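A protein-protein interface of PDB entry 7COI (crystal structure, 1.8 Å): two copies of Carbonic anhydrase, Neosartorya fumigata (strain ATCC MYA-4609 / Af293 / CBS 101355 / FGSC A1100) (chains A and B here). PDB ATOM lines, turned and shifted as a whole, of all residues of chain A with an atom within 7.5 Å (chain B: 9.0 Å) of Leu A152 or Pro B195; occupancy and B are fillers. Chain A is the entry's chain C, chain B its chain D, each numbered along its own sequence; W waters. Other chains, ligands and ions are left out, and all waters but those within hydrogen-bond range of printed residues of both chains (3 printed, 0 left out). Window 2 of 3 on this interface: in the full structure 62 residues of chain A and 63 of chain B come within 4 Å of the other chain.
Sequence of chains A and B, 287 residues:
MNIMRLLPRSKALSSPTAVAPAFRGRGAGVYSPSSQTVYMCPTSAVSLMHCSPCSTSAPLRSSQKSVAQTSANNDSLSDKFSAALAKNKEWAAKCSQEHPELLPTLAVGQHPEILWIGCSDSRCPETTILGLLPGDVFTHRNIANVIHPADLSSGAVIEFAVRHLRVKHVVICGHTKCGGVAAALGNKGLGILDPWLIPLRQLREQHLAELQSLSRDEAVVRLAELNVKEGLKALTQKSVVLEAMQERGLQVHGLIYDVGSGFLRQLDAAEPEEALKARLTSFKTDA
Water W3 lies within hydrogen-bond range of the side-chain carboxylate of Asp B151, the side-chain hydroxyl of Ser A153 and the side-chain amide nitrogen of Asn B142.
Water W2 lies within hydrogen-bond range of OD2 of Asp A151 (2.6 Å), NE2 of His A140 (2.7 Å) and OG of Ser B153 (2.8 Å).
Water W1 lies within hydrogen-bond range of the backbone carbonyl oxygen of Ser A153 (2.8 Å) and the backbone NH of Ile B143 (2.9 Å).
Ser A153 touches its own counterpart, Ser B153.
Positions printed for both chains: 148, 151, 152 and 153.
Of the 12 printed residues of chain A, 5 touch a printed residue of chain B.
Printed residues of chain A that touch a printed residue of chain B: Leu A152, Ser A153, Gly A155, Ala A156 and Val A157.
Hydrophobic or aromatic side chains of chain A within 4 Å of the printed part of chain B: Leu A152, Ala A156 and Val A157.
Among the printed residues, 11 pairs touch across the chains.
The backbone NH of Ser A153 is in hydrogen-bond range of the side-chain carboxylate of Asp A151 (3.0 Å).
The backbone carbonyl oxygen (O) of Val B146 is in hydrogen-bond range of the side-chain amide nitrogen (ND2) of Asn B142, at 3.0 Å.
The backbone carbonyl oxygen of Ile B143 is in hydrogen-bond range of the indole nitrogen of Trp B196, 2.8 Å away.
A ring nitrogen (NE2) of His B148 lies within hydrogen-bond range of the backbone carbonyl oxygen (O) of Trp B196 (2.8 Å).
OD1 of Asp B151 lies within hydrogen-bond range of N of Ser B153 (3.0 Å).
Of chain B, only Ile B192, Pro B195 and Trp B196 come within 4 Å of Leu A152.
Printed residues of chain A within 4 Å of Pro B195: Leu A152.
No residue of chain B comes within 4 Å of Asp A151.
Ser A153 touches three residues of chain B.
Printed residues of chain B within 4 Å of Gly A155: Ile B192.
Of the printed residues of chain B, Ala A156 touches Ile B143 (3.9 Å), Leu B193 (3.7 Å) and Trp B196 (3.8 Å).
Printed residues of chain B within 4 Å of Val A157: Ile B143.
Printed residues of chain A within 4 Å of Ile B143: Ala A156 and Val A157.
Of the printed residues of chain A, Ser B153 touches Ser A153.
Asp B194 touches none of the printed residues of chain A.
Leu B152 touches none of the printed residues of chain A.
The nearest printed residue of chain B that does not touch Leu A152 is Asp B151 (6.2 Å).
Among the printed residues, pairs that only touch across the chains: Leu A152 with Ile B192 (3.4 Å), Ser A153 with Trp B196 (3.6 Å), Ser A153 with Asn B142 (3.7 Å), Gly A155 with Ile B192 (3.7 Å), Ala A156 with Leu B193 (3.7 Å), Ala A156 with Trp B196 (3.8 Å), Ser A153 with Ser B153 (3.9 Å), Val A157 with Ile B143 (3.9 Å), Ala A156 with Ile B143 (3.9 Å), Leu A152 with Trp B196 (3.9 Å) and Leu A152 with Pro B195 (3.9 Å).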
ATOM      1  N   HIS A 140      22.820   2.747 -13.769  1.00  0.00           N
ATOM      2  CA  HIS A 140      21.826   1.788 -13.234  1.00  0.00           C
ATOM      3  C   HIS A 140      22.354   1.176 -11.954  1.00  0.00           C
ATOM      4  O   HIS A 140      23.476   0.625 -11.943  1.00  0.00           O
ATOM      5  CB  HIS A 140      21.510   0.730 -14.296  1.00  0.00           C
ATOM      6  CG  HIS A 140      20.350  -0.145 -13.968  1.00  0.00           C
ATOM      7  ND1 HIS A 140      19.114   0.366 -13.663  1.00  0.00           N
ATOM      8  CD2 HIS A 140      20.216  -1.490 -13.928  1.00  0.00           C
ATOM      9  CE1 HIS A 140      18.260  -0.634 -13.479  1.00  0.00           C
ATOM     10  NE2 HIS A 140      18.910  -1.779 -13.605  1.00  0.00           N
ATOM     11  N   HIS A 148      19.674  -9.868 -14.722  1.00  0.00           N
ATOM     12  CA  HIS A 148      18.705 -10.875 -15.213  1.00  0.00           C
ATOM     13  C   HIS A 148      18.599 -10.640 -16.693  1.00  0.00           C
ATOM     14  O   HIS A 148      18.283  -9.519 -17.105  1.00  0.00           O
ATOM     15  CB  HIS A 148      17.322 -10.717 -14.562  1.00  0.00           C
ATOM     16  CG  HIS A 148      17.305 -11.014 -13.106  1.00  0.00           C
ATOM     17  ND1 HIS A 148      16.922 -12.239 -12.605  1.00  0.00           N
ATOM     18  CD2 HIS A 148      17.548 -10.231 -12.044  1.00  0.00           C
ATOM     19  CE1 HIS A 148      16.945 -12.195 -11.305  1.00  0.00           C
ATOM     20  NE2 HIS A 148      17.356 -10.982 -10.928  1.00  0.00           N
ATOM     21  N   PRO A 149      18.841 -11.665 -17.541  1.00  0.00           N
ATOM     22  CA  PRO A 149      18.830 -11.454 -18.989  1.00  0.00           C
ATOM     23  C   PRO A 149      17.583 -10.740 -19.524  1.00  0.00           C
ATOM     24  O   PRO A 149      17.725  -9.878 -20.355  1.00  0.00           O
ATOM     25  CB  PRO A 149      18.866 -12.892 -19.541  1.00  0.00           C
ATOM     26  CG  PRO A 149      19.636 -13.655 -18.469  1.00  0.00           C
ATOM     27  CD  PRO A 149      19.177 -13.047 -17.157  1.00  0.00           C
ATOM     28  N   ALA A 150      16.405 -11.094 -19.035  1.00  0.00           N
ATOM     29  CA  ALA A 150      15.126 -10.568 -19.551  1.00  0.00           C
ATOM     30  C   ALA A 150      14.526  -9.492 -18.632  1.00  0.00           C
ATOM     31  O   ALA A 150      13.320  -9.146 -18.794  1.00  0.00           O
ATOM     32  CB  ALA A 150      14.172 -11.695 -19.791  1.00  0.00           C
ATOM     33  N   ASP A 151      15.313  -8.937 -17.721  1.00  0.00           N
ATOM     34  CA  ASP A 151      14.890  -7.778 -16.883  1.00  0.00           C
ATOM     35  C   ASP A 151      14.748  -6.547 -17.796  1.00  0.00           C
ATOM     36  O   ASP A 151      15.740  -6.106 -18.405  1.00  0.00           O
ATOM     37  CB  ASP A 151      15.902  -7.546 -15.770  1.00  0.00           C
ATOM     38  CG  ASP A 151      15.687  -6.244 -15.017  1.00  0.00           C
ATOM     39  OD1 ASP A 151      14.540  -5.835 -14.875  1.00  0.00           O
ATOM     40  OD2 ASP A 151      16.671  -5.676 -14.617  1.00  0.00           O
ATOM     41  N   LEU A 152      13.558  -5.980 -17.895  1.00  0.00           N
ATOM     42  CA  LEU A 152      13.346  -4.767 -18.713  1.00  0.00           C
ATOM     43  C   LEU A 152      14.021  -3.552 -18.095  1.00  0.00           C
ATOM     44  O   LEU A 152      14.354  -2.643 -18.847  1.00  0.00           O
ATOM     45  CB  LEU A 152      11.849  -4.493 -18.849  1.00  0.00           C
ATOM     46  CG  LEU A 152      11.104  -5.439 -19.780  1.00  0.00           C
ATOM     47  CD1 LEU A 152       9.672  -4.954 -19.921  1.00  0.00           C
ATOM     48  CD2 LEU A 152      11.780  -5.501 -21.144  1.00  0.00           C
ATOM     49  N   SER A 153      14.179  -3.489 -16.774  1.00  0.00           N
ATOM     50  CA  SER A 153      14.808  -2.317 -16.112  1.00  0.00           C
ATOM     51  C   SER A 153      16.247  -2.162 -16.601  1.00  0.00           C
ATOM     52  O   SER A 153      16.574  -1.094 -17.213  1.00  0.00           O
ATOM     53  CB  SER A 153      14.756  -2.393 -14.643  1.00  0.00           C
ATOM     54  OG  SER A 153      15.201  -1.174 -14.066  1.00  0.00           O
ATOM     55  N   SER A 154      17.083  -3.179 -16.419  1.00  0.00           N
ATOM     56  CA  SER A 154      18.476  -3.138 -16.925  1.00  0.00           C
ATOM     57  C   SER A 154      18.460  -3.152 -18.452  1.00  0.00           C
ATOM     58  O   SER A 154      19.317  -2.470 -19.041  1.00  0.00           O
ATOM     59  CB  SER A 154      19.338  -4.227 -16.337  1.00  0.00           C
ATOM     60  OG  SER A 154      18.839  -5.488 -16.691  1.00  0.00           O
ATOM     61  N   GLY A 155      17.551  -3.913 -19.079  1.00  0.00           N
ATOM     62  CA  GLY A 155      17.468  -4.013 -20.543  1.00  0.00           C
ATOM     63  C   GLY A 155      17.286  -2.654 -21.187  1.00  0.00           C
ATOM     64  O   GLY A 155      17.969  -2.334 -22.194  1.00  0.00           O
ATOM     65  N   ALA A 156      16.354  -1.865 -20.668  1.00  0.00           N
ATOM     66  CA  ALA A 156      16.047  -0.518 -21.198  1.00  0.00           C
ATOM     67  C   ALA A 156      17.248   0.422 -20.973  1.00  0.00           C
ATOM     68  O   ALA A 156      17.575   1.201 -21.879  1.00  0.00           O
ATOM     69  CB  ALA A 156      14.770  -0.030 -20.555  1.00  0.00           C
ATOM     70  N   VAL A 157      17.908   0.351 -19.830  1.00  0.00           N
ATOM     71  CA  VAL A 157      19.100   1.194 -19.536  1.00  0.00           C
ATOM     72  C   VAL A 157      20.183   0.869 -20.562  1.00  0.00           C
ATOM     73  O   VAL A 157      20.785   1.805 -21.133  1.00  0.00           O
ATOM     74  CB  VAL A 157      19.608   1.001 -18.109  1.00  0.00           C
ATOM     75  CG1 VAL A 157      21.016   1.567 -17.957  1.00  0.00           C
ATOM     76  CG2 VAL A 157      18.601   1.596 -17.106  1.00  0.00           C
ATOM     77  N   ILE A 158      20.433  -0.423 -20.773  1.00  0.00           N
ATOM     78  CA  ILE A 158      21.523  -0.862 -21.687  1.00  0.00           C
ATOM     79  C   ILE A 158      21.200  -0.404 -23.105  1.00  0.00           C
ATOM     80  O   ILE A 158      22.101   0.130 -23.775  1.00  0.00           O
ATOM     81  CB  ILE A 158      21.739  -2.378 -21.559  1.00  0.00           C
ATOM     82  CG1 ILE A 158      22.338  -2.682 -20.185  1.00  0.00           C
ATOM     83  CG2 ILE A 158      22.630  -2.870 -22.705  1.00  0.00           C
ATOM     84  CD1 ILE A 158      22.239  -4.104 -19.763  1.00  0.00           C
ATOM     85  N   ASN B 142      16.871   4.225 -12.986  1.00  0.00           N
ATOM     86  CA  ASN B 142      16.353   3.491 -14.160  1.00  0.00           C
ATOM     87  C   ASN B 142      15.954   4.521 -15.202  1.00  0.00           C
ATOM     88  O   ASN B 142      16.060   5.757 -14.951  1.00  0.00           O
ATOM     89  CB  ASN B 142      15.257   2.492 -13.769  1.00  0.00           C
ATOM     90  CG  ASN B 142      13.989   3.164 -13.291  1.00  0.00           C
ATOM     91  OD1 ASN B 142      13.761   4.325 -13.634  1.00  0.00           O
ATOM     92  ND2 ASN B 142      13.144   2.448 -12.543  1.00  0.00           N
ATOM     93  N   ILE B 143      15.454   4.072 -16.355  1.00  0.00           N
ATOM     94  CA  ILE B 143      15.024   5.030 -17.402  1.00  0.00           C
ATOM     95  C   ILE B 143      13.765   5.777 -16.930  1.00  0.00           C
ATOM     96  O   ILE B 143      12.694   5.159 -16.742  1.00  0.00           O
ATOM     97  CB  ILE B 143      14.791   4.354 -18.756  1.00  0.00           C
ATOM     98  CG1 ILE B 143      16.074   3.707 -19.279  1.00  0.00           C
ATOM     99  CG2 ILE B 143      14.194   5.339 -19.732  1.00  0.00           C
ATOM    100  CD1 ILE B 143      17.262   4.646 -19.411  1.00  0.00           C
ATOM    101  N   VAL B 146      10.821   5.398 -13.520  1.00  0.00           N
ATOM    102  CA  VAL B 146       9.476   4.796 -13.667  1.00  0.00           C
ATOM    103  C   VAL B 146       9.326   3.709 -12.598  1.00  0.00           C
ATOM    104  O   VAL B 146      10.224   2.864 -12.422  1.00  0.00           O
ATOM    105  CB  VAL B 146       9.256   4.251 -15.076  1.00  0.00           C
ATOM    106  CG1 VAL B 146       7.942   3.485 -15.166  1.00  0.00           C
ATOM    107  CG2 VAL B 146       9.311   5.370 -16.095  1.00  0.00           C
ATOM    108  N   HIS B 148       7.135   0.679 -12.169  1.00  0.00           N
ATOM    109  CA  HIS B 148       6.179  -0.378 -12.583  1.00  0.00           C
ATOM    110  C   HIS B 148       5.833  -1.102 -11.311  1.00  0.00           C
ATOM    111  O   HIS B 148       6.735  -1.573 -10.615  1.00  0.00           O
ATOM    112  CB  HIS B 148       6.812  -1.345 -13.590  1.00  0.00           C
ATOM    113  CG  HIS B 148       7.127  -0.742 -14.915  1.00  0.00           C
ATOM    114  ND1 HIS B 148       6.298  -0.852 -16.009  1.00  0.00           N
ATOM    115  CD2 HIS B 148       8.203  -0.066 -15.354  1.00  0.00           C
ATOM    116  CE1 HIS B 148       6.855  -0.268 -17.058  1.00  0.00           C
ATOM    117  NE2 HIS B 148       8.012   0.224 -16.686  1.00  0.00           N
ATOM    118  N   ASP B 151       7.497  -4.557 -10.938  1.00  0.00           N
ATOM    119  CA  ASP B 151       8.929  -4.647 -11.356  1.00  0.00           C
ATOM    120  C   ASP B 151       9.734  -5.195 -10.179  1.00  0.00           C
ATOM    121  O   ASP B 151       9.756  -4.575  -9.117  1.00  0.00           O
ATOM    122  CB  ASP B 151       9.396  -3.276 -11.852  1.00  0.00           C
ATOM    123  CG  ASP B 151      10.900  -3.161 -11.991  1.00  0.00           C
ATOM    124  OD1 ASP B 151      11.519  -4.143 -12.369  1.00  0.00           O
ATOM    125  OD2 ASP B 151      11.415  -2.103 -11.695  1.00  0.00           O
ATOM    126  N   LEU B 152      10.399  -6.339 -10.331  1.00  0.00           N
ATOM    127  CA  LEU B 152      11.245  -6.882  -9.241  1.00  0.00           C
ATOM    128  C   LEU B 152      12.474  -6.016  -8.994  1.00  0.00           C
ATOM    129  O   LEU B 152      12.959  -6.026  -7.893  1.00  0.00           O
ATOM    130  CB  LEU B 152      11.719  -8.305  -9.551  1.00  0.00           C
ATOM    131  CG  LEU B 152      10.655  -9.377  -9.492  1.00  0.00           C
ATOM    132  CD1 LEU B 152      11.293 -10.726  -9.795  1.00  0.00           C
ATOM    133  CD2 LEU B 152       9.964  -9.364  -8.138  1.00  0.00           C
ATOM    134  N   SER B 153      12.991  -5.303  -9.985  1.00  0.00           N
ATOM    135  CA  SER B 153      14.193  -4.458  -9.800  1.00  0.00           C
ATOM    136  C   SER B 153      13.914  -3.361  -8.756  1.00  0.00           C
ATOM    137  O   SER B 153      14.583  -3.333  -7.698  1.00  0.00           O
ATOM    138  CB  SER B 153      14.679  -3.873 -11.084  1.00  0.00           C
ATOM    139  OG  SER B 153      15.921  -3.212 -10.869  1.00  0.00           O
ATOM    140  N   GLY B 189       9.140   3.937 -32.450  1.00  0.00           N
ATOM    141  CA  GLY B 189       9.420   2.642 -31.796  1.00  0.00           C
ATOM    142  C   GLY B 189      10.865   2.550 -31.363  1.00  0.00           C
ATOM    143  O   GLY B 189      11.718   2.881 -32.164  1.00  0.00           O
ATOM    144  N   LEU B 190      11.147   2.135 -30.125  1.00  0.00           N
ATOM    145  CA  LEU B 190      12.501   2.175 -29.518  1.00  0.00           C
ATOM    146  C   LEU B 190      12.853   0.794 -28.941  1.00  0.00           C
ATOM    147  O   LEU B 190      13.665   0.717 -28.030  1.00  0.00           O
ATOM    148  CB  LEU B 190      12.524   3.262 -28.440  1.00  0.00           C
ATOM    149  CG  LEU B 190      12.344   4.678 -28.975  1.00  0.00           C
ATOM    150  CD1 LEU B 190      12.169   5.689 -27.858  1.00  0.00           C
ATOM    151  CD2 LEU B 190      13.509   5.061 -29.885  1.00  0.00           C
ATOM    152  N   GLY B 191      12.285  -0.248 -29.529  1.00  0.00           N
ATOM    153  CA  GLY B 191      12.617  -1.636 -29.180  1.00  0.00           C
ATOM    154  C   GLY B 191      12.223  -1.932 -27.741  1.00  0.00           C
ATOM    155  O   GLY B 191      11.046  -1.699 -27.373  1.00  0.00           O
ATOM    156  N   ILE B 192      13.170  -2.432 -26.954  1.00  0.00           N
ATOM    157  CA  ILE B 192      12.882  -2.909 -25.567  1.00  0.00           C
ATOM    158  C   ILE B 192      12.452  -1.727 -24.697  1.00  0.00           C
ATOM    159  O   ILE B 192      11.790  -1.972 -23.668  1.00  0.00           O
ATOM    160  CB  ILE B 192      14.095  -3.639 -24.992  1.00  0.00           C
ATOM    161  CG1 ILE B 192      13.728  -4.508 -23.794  1.00  0.00           C
ATOM    162  CG2 ILE B 192      15.237  -2.696 -24.665  1.00  0.00           C
ATOM    163  CD1 ILE B 192      14.885  -5.416 -23.365  1.00  0.00           C
ATOM    164  N   LEU B 193      12.750  -0.480 -25.100  1.00  0.00           N
ATOM    165  CA  LEU B 193      12.278   0.706 -24.348  1.00  0.00           C
ATOM    166  C   LEU B 193      10.757   0.809 -24.404  1.00  0.00           C
ATOM    167  O   LEU B 193      10.200   1.410 -23.488  1.00  0.00           O
ATOM    168  CB  LEU B 193      12.933   1.976 -24.880  1.00  0.00           C
ATOM    169  CG  LEU B 193      14.362   2.170 -24.374  1.00  0.00           C
ATOM    170  CD1 LEU B 193      15.161   3.045 -25.327  1.00  0.00           C
ATOM    171  CD2 LEU B 193      14.364   2.784 -22.977  1.00  0.00           C
ATOM    172  N   ASP B 194      10.097   0.272 -25.422  1.00  0.00           N
ATOM    173  CA  ASP B 194       8.645   0.512 -25.616  1.00  0.00           C
ATOM    174  C   ASP B 194       7.845  -0.044 -24.437  1.00  0.00           C
ATOM    175  O   ASP B 194       7.038   0.669 -23.862  1.00  0.00           O
ATOM    176  CB  ASP B 194       8.144  -0.085 -26.931  1.00  0.00           C
ATOM    177  CG  ASP B 194       8.627   0.667 -28.161  1.00  0.00           C
ATOM    178  OD1 ASP B 194       9.365   1.710 -28.000  1.00  0.00           O
ATOM    179  OD2 ASP B 194       8.239   0.227 -29.274  1.00  0.00           O
ATOM    180  N   PRO B 195       7.973  -1.328 -24.037  1.00  0.00           N
ATOM    181  CA  PRO B 195       7.241  -1.791 -22.851  1.00  0.00           C
ATOM    182  C   PRO B 195       7.650  -1.002 -21.593  1.00  0.00           C
ATOM    183  O   PRO B 195       6.817  -0.761 -20.724  1.00  0.00           O
ATOM    184  CB  PRO B 195       7.573  -3.304 -22.784  1.00  0.00           C
ATOM    185  CG  PRO B 195       8.796  -3.497 -23.627  1.00  0.00           C
ATOM    186  CD  PRO B 195       8.708  -2.417 -24.699  1.00  0.00           C
ATOM    187  N   TRP B 196       8.934  -0.655 -21.481  1.00  0.00           N
ATOM    188  CA  TRP B 196       9.426   0.058 -20.279  1.00  0.00           C
ATOM    189  C   TRP B 196       8.671   1.384 -20.140  1.00  0.00           C
ATOM    190  O   TRP B 196       8.332   1.780 -18.987  1.00  0.00           O
ATOM    191  CB  TRP B 196      10.930   0.286 -20.338  1.00  0.00           C
ATOM    192  CG  TRP B 196      11.370   1.022 -19.118  1.00  0.00           C
ATOM    193  CD1 TRP B 196      11.603   2.363 -18.994  1.00  0.00           C
ATOM    194  CD2 TRP B 196      11.465   0.453 -17.805  1.00  0.00           C
ATOM    195  NE1 TRP B 196      11.877   2.653 -17.689  1.00  0.00           N
ATOM    196  CE2 TRP B 196      11.774   1.518 -16.933  1.00  0.00           C
ATOM    197  CE3 TRP B 196      11.304  -0.826 -17.280  1.00  0.00           C
ATOM    198  CZ2 TRP B 196      11.987   1.312 -15.577  1.00  0.00           C
ATOM    199  CZ3 TRP B 196      11.488  -1.027 -15.923  1.00  0.00           C
ATOM    200  CH2 TRP B 196      11.848   0.041 -15.095  1.00  0.00           C
ATOM    201  N   LEU B 197       8.398   2.054 -21.255  1.00  0.00           N
ATOM    202  CA  LEU B 197       7.833   3.428 -21.249  1.00  0.00           C
ATOM    203  C   LEU B 197       6.315   3.416 -21.185  1.00  0.00           C
ATOM    204  O   LEU B 197       5.726   4.511 -21.093  1.00  0.00           O
ATOM    205  CB  LEU B 197       8.303   4.193 -22.494  1.00  0.00           C
ATOM    206  CG  LEU B 197       9.811   4.441 -22.547  1.00  0.00           C
ATOM    207  CD1 LEU B 197      10.222   5.029 -23.886  1.00  0.00           C
ATOM    208  CD2 LEU B 197      10.271   5.327 -21.405  1.00  0.00           C
ATOM    209  N   ILE B 198       5.668   2.242 -21.166  1.00  0.00           N
ATOM    210  CA  ILE B 198       4.187   2.196 -21.139  1.00  0.00           C
ATOM    211  C   ILE B 198       3.585   3.118 -20.063  1.00  0.00           C
ATOM    212  O   ILE B 198       2.601   3.809 -20.345  1.00  0.00           O
ATOM    213  CB  ILE B 198       3.666   0.749 -21.050  1.00  0.00           C
ATOM    214  CG1 ILE B 198       3.833   0.050 -22.406  1.00  0.00           C
ATOM    215  CG2 ILE B 198       2.227   0.738 -20.597  1.00  0.00           C
ATOM    216  CD1 ILE B 198       3.654  -1.458 -22.352  1.00  0.00           C
ATOM    217  N   PRO B 199       4.063   3.133 -18.801  1.00  0.00           N
ATOM    218  CA  PRO B 199       3.428   3.967 -17.767  1.00  0.00           C
ATOM    219  C   PRO B 199       3.387   5.460 -18.107  1.00  0.00           C
ATOM    220  O   PRO B 199       2.413   6.117 -17.745  1.00  0.00           O
ATOM    221  CB  PRO B 199       4.259   3.703 -16.510  1.00  0.00           C
ATOM    222  CG  PRO B 199       4.774   2.295 -16.739  1.00  0.00           C
ATOM    223  CD  PRO B 199       5.098   2.259 -18.218  1.00  0.00           C
ATOM    224  N   LEU B 200       4.418   5.928 -18.788  1.00  0.00           N
ATOM    225  CA  LEU B 200       4.496   7.334 -19.278  1.00  0.00           C
ATOM    226  C   LEU B 200       3.459   7.560 -20.368  1.00  0.00           C
ATOM    227  O   LEU B 200       2.788   8.597 -20.319  1.00  0.00           O
ATOM    228  CB  LEU B 200       5.914   7.600 -19.761  1.00  0.00           C
ATOM    229  CG  LEU B 200       6.952   7.739 -18.652  1.00  0.00           C
ATOM    230  CD1 LEU B 200       8.344   7.725 -19.229  1.00  0.00           C
ATOM    231  CD2 LEU B 200       6.717   9.035 -17.878  1.00  0.00           C
ATOM    232  N   ARG B 201       3.288   6.617 -21.300  1.00  0.00           N
ATOM    233  CA  ARG B 201       2.258   6.714 -22.348  1.00  0.00           C
ATOM    234  C   ARG B 201       0.875   6.610 -21.722  1.00  0.00           C
ATOM    235  O   ARG B 201      -0.027   7.265 -22.238  1.00  0.00           O
ATOM    236  CB  ARG B 201       2.513   5.703 -23.469  1.00  0.00           C
ATOM    237  CG  ARG B 201       3.744   6.005 -24.293  1.00  0.00           C
ATOM    238  CD  ARG B 201       3.918   4.996 -25.412  1.00  0.00           C
ATOM    239  NE  ARG B 201       5.141   5.282 -26.149  1.00  0.00           N
ATOM    240  CZ  ARG B 201       5.219   6.177 -27.141  1.00  0.00           C
ATOM    241  NH1 ARG B 201       4.147   6.869 -27.505  1.00  0.00           N
ATOM    242  NH2 ARG B 201       6.370   6.378 -27.741  1.00  0.00           N
ATOM    243  N   GLN B 202       0.688   5.858 -20.622  1.00  0.00           N
ATOM    244  CA  GLN B 202      -0.629   5.786 -19.954  1.00  0.00           C
ATOM    245  C   GLN B 202      -0.979   7.181 -19.392  1.00  0.00           C
ATOM    246  O   GLN B 202      -2.138   7.622 -19.521  1.00  0.00           O
ATOM    247  CB  GLN B 202      -0.618   4.741 -18.836  1.00  0.00           C
ATOM    248  CG  GLN B 202      -0.477   3.308 -19.367  1.00  0.00           C
ATOM    249  CD  GLN B 202      -0.384   2.310 -18.240  1.00  0.00           C
ATOM    250  OE1 GLN B 202       0.349   2.490 -17.258  1.00  0.00           O
ATOM    251  NE2 GLN B 202      -1.172   1.255 -18.346  1.00  0.00           N
HETATM  252  O   HOH W   1      15.059   1.223 -16.946  1.00  0.00           O
HETATM  253  O   HOH W   2      17.707  -4.102 -12.777  1.00  0.00           O
HETATM  254  O   HOH W   3      13.394  -0.437 -12.072  1.00  0.00           O
